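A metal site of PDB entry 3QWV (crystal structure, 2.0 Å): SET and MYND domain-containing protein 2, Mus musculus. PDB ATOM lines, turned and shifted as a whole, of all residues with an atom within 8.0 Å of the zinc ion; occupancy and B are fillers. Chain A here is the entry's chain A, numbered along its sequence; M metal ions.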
ATOM      1  N   LYS A  64       8.883  27.964  -8.657  1.00  0.00           N
ATOM      2  CA  LYS A  64       9.332  27.324  -9.894  1.00  0.00           C
ATOM      3  C   LYS A  64       8.220  26.629 -10.671  1.00  0.00           C
ATOM      4  O   LYS A  64       7.210  26.210 -10.087  1.00  0.00           O
ATOM      5  CB  LYS A  64      10.534  26.394  -9.656  1.00  0.00           C
ATOM      6  CG  LYS A  64      10.237  25.073  -8.961  1.00  0.00           C
ATOM      7  CD  LYS A  64      11.492  24.233  -8.801  1.00  0.00           C
ATOM      8  CE  LYS A  64      12.113  24.340  -7.434  1.00  0.00           C
ATOM      9  NZ  LYS A  64      12.212  23.015  -6.769  1.00  0.00           N
ATOM     10  N   CYS A  65       8.423  26.477 -12.008  1.00  0.00           N
ATOM     11  CA  CYS A  65       7.501  25.738 -12.855  1.00  0.00           C
ATOM     12  C   CYS A  65       7.731  24.263 -12.436  1.00  0.00           C
ATOM     13  O   CYS A  65       8.878  23.824 -12.340  1.00  0.00           O
ATOM     14  CB  CYS A  65       7.836  25.951 -14.327  1.00  0.00           C
ATOM     15  SG  CYS A  65       6.951  24.830 -15.444  1.00  0.00           S
ATOM     16  N   GLY A  66       6.650  23.572 -12.088  1.00  0.00           N
ATOM     17  CA  GLY A  66       6.716  22.190 -11.615  1.00  0.00           C
ATOM     18  C   GLY A  66       7.216  21.173 -12.619  1.00  0.00           C
ATOM     19  O   GLY A  66       7.734  20.127 -12.243  1.00  0.00           O
ATOM     20  N   ARG A  67       7.073  21.478 -13.928  1.00  0.00           N
ATOM     21  CA  ARG A  67       7.523  20.556 -14.974  1.00  0.00           C
ATOM     22  C   ARG A  67       9.016  20.596 -15.260  1.00  0.00           C
ATOM     23  O   ARG A  67       9.689  19.587 -15.048  1.00  0.00           O
ATOM     24  CB  ARG A  67       6.674  20.679 -16.242  1.00  0.00           C
ATOM     25  CG  ARG A  67       6.298  19.312 -16.785  1.00  0.00           C
ATOM     26  CD  ARG A  67       5.332  19.375 -17.940  1.00  0.00           C
ATOM     27  NE  ARG A  67       5.692  18.399 -18.968  1.00  0.00           N
ATOM     28  CZ  ARG A  67       6.374  18.690 -20.068  1.00  0.00           C
ATOM     29  NH1 ARG A  67       6.783  19.936 -20.301  1.00  0.00           N
ATOM     30  NH2 ARG A  67       6.661  17.739 -20.953  1.00  0.00           N
ATOM     31  N   CYS A  68       9.551  21.745 -15.691  1.00  0.00           N
ATOM     32  CA  CYS A  68      10.952  21.902 -16.016  1.00  0.00           C
ATOM     33  C   CYS A  68      11.805  22.241 -14.812  1.00  0.00           C
ATOM     34  O   CYS A  68      13.002  21.956 -14.817  1.00  0.00           O
ATOM     35  CB  CYS A  68      11.138  22.947 -17.117  1.00  0.00           C
ATOM     36  SG  CYS A  68      10.673  24.628 -16.606  1.00  0.00           S
ATOM     37  N   LYS A  69      11.218  22.963 -13.822  1.00  0.00           N
ATOM     38  CA  LYS A  69      11.939  23.424 -12.629  1.00  0.00           C
ATOM     39  C   LYS A  69      13.075  24.415 -13.000  1.00  0.00           C
ATOM     40  O   LYS A  69      14.017  24.603 -12.227  1.00  0.00           O
ATOM     41  CB  LYS A  69      12.413  22.231 -11.764  1.00  0.00           C
ATOM     42  CG  LYS A  69      11.258  21.376 -11.240  1.00  0.00           C
ATOM     43  CD  LYS A  69      11.698  20.129 -10.481  1.00  0.00           C
ATOM     44  CE  LYS A  69      10.561  19.154 -10.237  1.00  0.00           C
ATOM     45  NZ  LYS A  69      10.201  18.403 -11.474  1.00  0.00           N
ATOM     46  N   GLN A  70      12.942  25.086 -14.173  1.00  0.00           N
ATOM     47  CA  GLN A  70      13.918  26.031 -14.728  1.00  0.00           C
ATOM     48  C   GLN A  70      13.372  27.470 -14.831  1.00  0.00           C
ATOM     49  O   GLN A  70      14.176  28.408 -14.909  1.00  0.00           O
ATOM     50  CB  GLN A  70      14.401  25.545 -16.088  1.00  0.00           C
ATOM     51  CG  GLN A  70      15.794  26.025 -16.471  1.00  0.00           C
ATOM     52  CD  GLN A  70      16.902  25.036 -16.186  1.00  0.00           C
ATOM     53  OE1 GLN A  70      16.680  23.815 -16.063  1.00  0.00           O
ATOM     54  NE2 GLN A  70      18.134  25.534 -16.152  1.00  0.00           N
ATOM     55  N   ALA A  71      12.037  27.652 -14.828  1.00  0.00           N
ATOM     56  CA  ALA A  71      11.412  28.983 -14.888  1.00  0.00           C
ATOM     57  C   ALA A  71      10.877  29.278 -13.512  1.00  0.00           C
ATOM     58  O   ALA A  71      10.259  28.401 -12.909  1.00  0.00           O
ATOM     59  CB  ALA A  71      10.287  29.004 -15.910  1.00  0.00           C
ATOM     60  N   PHE A  72      11.129  30.498 -13.015  1.00  0.00           N
ATOM     61  CA  PHE A  72      10.742  30.963 -11.677  1.00  0.00           C
ATOM     62  C   PHE A  72       9.958  32.242 -11.801  1.00  0.00           C
ATOM     63  O   PHE A  72      10.273  33.097 -12.634  1.00  0.00           O
ATOM     64  CB  PHE A  72      11.984  31.168 -10.808  1.00  0.00           C
ATOM     65  CG  PHE A  72      12.827  29.948 -10.535  1.00  0.00           C
ATOM     66  CD1 PHE A  72      13.716  29.460 -11.496  1.00  0.00           C
ATOM     67  CD2 PHE A  72      12.791  29.314  -9.290  1.00  0.00           C
ATOM     68  CE1 PHE A  72      14.519  28.354 -11.229  1.00  0.00           C
ATOM     69  CE2 PHE A  72      13.609  28.206  -9.023  1.00  0.00           C
ATOM     70  CZ  PHE A  72      14.470  27.733  -9.991  1.00  0.00           C
ATOM     71  N   TYR A  73       8.895  32.361 -11.000  1.00  0.00           N
ATOM     72  CA  TYR A  73       7.905  33.427 -11.030  1.00  0.00           C
ATOM     73  C   TYR A  73       7.556  33.987  -9.683  1.00  0.00           C
ATOM     74  O   TYR A  73       7.698  33.302  -8.678  1.00  0.00           O
ATOM     75  CB  TYR A  73       6.625  32.876 -11.665  1.00  0.00           C
ATOM     76  CG  TYR A  73       6.832  32.378 -13.078  1.00  0.00           C
ATOM     77  CD1 TYR A  73       7.006  33.270 -14.124  1.00  0.00           C
ATOM     78  CD2 TYR A  73       6.881  31.013 -13.355  1.00  0.00           C
ATOM     79  CE1 TYR A  73       7.183  32.820 -15.430  1.00  0.00           C
ATOM     80  CE2 TYR A  73       7.063  30.551 -14.665  1.00  0.00           C
ATOM     81  CZ  TYR A  73       7.226  31.456 -15.693  1.00  0.00           C
ATOM     82  OH  TYR A  73       7.395  31.065 -16.993  1.00  0.00           O
ATOM     83  N   GLN A  79       3.264  33.437 -13.606  1.00  0.00           N
ATOM     84  CA  GLN A  79       3.399  32.139 -14.264  1.00  0.00           C
ATOM     85  C   GLN A  79       2.385  31.998 -15.407  1.00  0.00           C
ATOM     86  O   GLN A  79       2.769  31.535 -16.479  1.00  0.00           O
ATOM     87  CB  GLN A  79       3.267  30.991 -13.270  1.00  0.00           C
ATOM     88  CG  GLN A  79       3.517  29.609 -13.904  1.00  0.00           C
ATOM     89  CD  GLN A  79       3.401  28.477 -12.911  1.00  0.00           C
ATOM     90  OE1 GLN A  79       3.800  27.342 -13.174  1.00  0.00           O
ATOM     91  NE2 GLN A  79       2.863  28.756 -11.739  1.00  0.00           N
ATOM     92  N   TRP A  83       3.144  31.896 -19.496  1.00  0.00           N
ATOM     93  CA  TRP A  83       2.875  30.570 -20.086  1.00  0.00           C
ATOM     94  C   TRP A  83       2.853  30.527 -21.627  1.00  0.00           C
ATOM     95  O   TRP A  83       3.523  29.657 -22.147  1.00  0.00           O
ATOM     96  CB  TRP A  83       1.685  29.863 -19.443  1.00  0.00           C
ATOM     97  CG  TRP A  83       1.356  28.528 -20.069  1.00  0.00           C
ATOM     98  CD1 TRP A  83       0.262  28.233 -20.827  1.00  0.00           C
ATOM     99  CD2 TRP A  83       2.143  27.338 -20.014  1.00  0.00           C
ATOM    100  NE1 TRP A  83       0.301  26.917 -21.215  1.00  0.00           N
ATOM    101  CE2 TRP A  83       1.440  26.330 -20.724  1.00  0.00           C
ATOM    102  CE3 TRP A  83       3.404  27.009 -19.473  1.00  0.00           C
ATOM    103  CZ2 TRP A  83       1.946  25.044 -20.898  1.00  0.00           C
ATOM    104  CZ3 TRP A  83       3.882  25.716 -19.613  1.00  0.00           C
ATOM    105  CH2 TRP A  83       3.162  24.750 -20.326  1.00  0.00           C
ATOM    106  N   HIS A  86       6.699  30.591 -22.211  1.00  0.00           N
ATOM    107  CA  HIS A  86       7.389  29.497 -21.542  1.00  0.00           C
ATOM    108  C   HIS A  86       7.030  28.121 -22.131  1.00  0.00           C
ATOM    109  O   HIS A  86       7.885  27.245 -22.152  1.00  0.00           O
ATOM    110  CB  HIS A  86       7.087  29.522 -20.029  1.00  0.00           C
ATOM    111  CG  HIS A  86       7.766  28.408 -19.294  1.00  0.00           C
ATOM    112  ND1 HIS A  86       9.144  28.293 -19.290  1.00  0.00           N
ATOM    113  CD2 HIS A  86       7.227  27.389 -18.593  1.00  0.00           C
ATOM    114  CE1 HIS A  86       9.406  27.180 -18.622  1.00  0.00           C
ATOM    115  NE2 HIS A  86       8.274  26.616 -18.161  1.00  0.00           N
ATOM    116  N   LYS A  87       5.781  27.945 -22.628  1.00  0.00           N
ATOM    117  CA  LYS A  87       5.353  26.668 -23.220  1.00  0.00           C
ATOM    118  C   LYS A  87       6.166  26.261 -24.462  1.00  0.00           C
ATOM    119  O   LYS A  87       6.199  25.086 -24.818  1.00  0.00           O
ATOM    120  CB  LYS A  87       3.834  26.621 -23.497  1.00  0.00           C
ATOM    121  CG  LYS A  87       3.370  27.431 -24.692  1.00  0.00           C
ATOM    122  CD  LYS A  87       1.882  27.309 -24.915  1.00  0.00           C
ATOM    123  CE  LYS A  87       1.503  27.913 -26.254  1.00  0.00           C
ATOM    124  NZ  LYS A  87       0.038  28.111 -26.386  1.00  0.00           N
ATOM    125  N   GLU A  89       9.355  26.559 -24.571  1.00  0.00           N
ATOM    126  CA  GLU A  89      10.638  26.116 -24.072  1.00  0.00           C
ATOM    127  C   GLU A  89      10.534  25.040 -22.983  1.00  0.00           C
ATOM    128  O   GLU A  89      11.493  24.286 -22.808  1.00  0.00           O
ATOM    129  CB  GLU A  89      11.420  27.319 -23.499  1.00  0.00           C
ATOM    130  CG  GLU A  89      11.483  28.523 -24.438  1.00  0.00           C
ATOM    131  CD  GLU A  89      12.234  29.726 -23.913  1.00  0.00           C
ATOM    132  OE1 GLU A  89      12.236  29.941 -22.680  1.00  0.00           O
ATOM    133  OE2 GLU A  89      12.855  30.436 -24.742  1.00  0.00           O
ATOM    134  N   CYS A  90       9.407  24.988 -22.245  1.00  0.00           N
ATOM    135  CA  CYS A  90       9.221  24.066 -21.124  1.00  0.00           C
ATOM    136  C   CYS A  90       9.553  22.595 -21.372  1.00  0.00           C
ATOM    137  O   CYS A  90      10.446  22.051 -20.712  1.00  0.00           O
ATOM    138  CB  CYS A  90       7.860  24.229 -20.454  1.00  0.00           C
ATOM    139  SG  CYS A  90       7.707  23.277 -18.921  1.00  0.00           S
ATOM    140  N   SER A  91       8.849  21.976 -22.330  1.00  0.00           N
ATOM    141  CA  SER A  91       9.065  20.574 -22.704  1.00  0.00           C
ATOM    142  C   SER A  91      10.470  20.332 -23.242  1.00  0.00           C
ATOM    143  O   SER A  91      11.037  19.277 -22.968  1.00  0.00           O
ATOM    144  CB  SER A  91       7.998  20.143 -23.704  1.00  0.00           C
ATOM    145  OG  SER A  91       8.058  18.754 -23.988  1.00  0.00           O
ATOM    146  N   SER A  92      11.050  21.299 -23.997  1.00  0.00           N
ATOM    147  CA  SER A  92      12.406  21.217 -24.551  1.00  0.00           C
ATOM    148  C   SER A  92      13.485  21.197 -23.472  1.00  0.00           C
ATOM    149  O   SER A  92      14.429  20.410 -23.560  1.00  0.00           O
ATOM    150  CB  SER A  92      12.664  22.347 -25.538  1.00  0.00           C
ATOM    151  OG  SER A  92      11.836  22.224 -26.696  1.00  0.00           O
ATOM    152  N   MET A  93      13.349  22.043 -22.427  1.00  0.00           N
ATOM    153  CA  MET A  93      14.289  22.091 -21.303  1.00  0.00           C
ATOM    154  C   MET A  93      14.298  20.754 -20.475  1.00  0.00           C
ATOM    155  O   MET A  93      15.321  20.427 -19.875  1.00  0.00           O
ATOM    156  CB  MET A  93      13.985  23.289 -20.378  1.00  0.00           C
ATOM    157  CG  MET A  93      14.515  24.619 -20.923  1.00  0.00           C
ATOM    158  SD  MET A  93      14.129  26.013 -19.819  1.00  0.00           S
ATOM    159  CE  MET A  93      12.438  26.191 -20.105  1.00  0.00           C
ATOM    160  N   VAL A  94      13.167  20.012 -20.462  1.00  0.00           N
ATOM    161  CA  VAL A  94      13.030  18.729 -19.756  1.00  0.00           C
ATOM    162  C   VAL A  94      13.819  17.644 -20.521  1.00  0.00           C
ATOM    163  O   VAL A  94      14.742  17.051 -19.969  1.00  0.00           O
ATOM    164  CB  VAL A  94      11.538  18.324 -19.570  1.00  0.00           C
ATOM    165  CG1 VAL A  94      11.389  16.926 -18.977  1.00  0.00           C
ATOM    166  CG2 VAL A  94      10.784  19.340 -18.718  1.00  0.00           C
HETATM  167 ZN    ZN M   1       8.477  24.751 -17.310  1.00  0.00          ZN
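The side-chain sulfur (SG) of Cys 68 sits close to the backbone NH (N) of Ala 71. N of Gln 70 lies close to SG of Cys 68 (3.4 Å). The side-chain sulfur (SG) of Cys 90 lies close to the guanidinium group (NH1) of Arg 67. The backbone NH of Arg 67 sits close to the side-chain sulfur of Cys 65, at 3.7 Å. The backbone NH (N) of Cys 65 is in hydrogen-bond range of the backbone carbonyl oxygen (O) of Ala 71 (2.8 Å).
The nearest printed residue that does not touch the zinc ion is Arg 67 (4.6 Å).
NE2 of His 86 is bound to the zinc ion (2.1 Å). The zinc ion is bound by SG of Cys 68. The zinc ion is bound by SG of Cys 90. The zinc ion is bound by SG of Cys 65, at 2.4 Å. The zinc ion has four donor atoms within binding distance.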
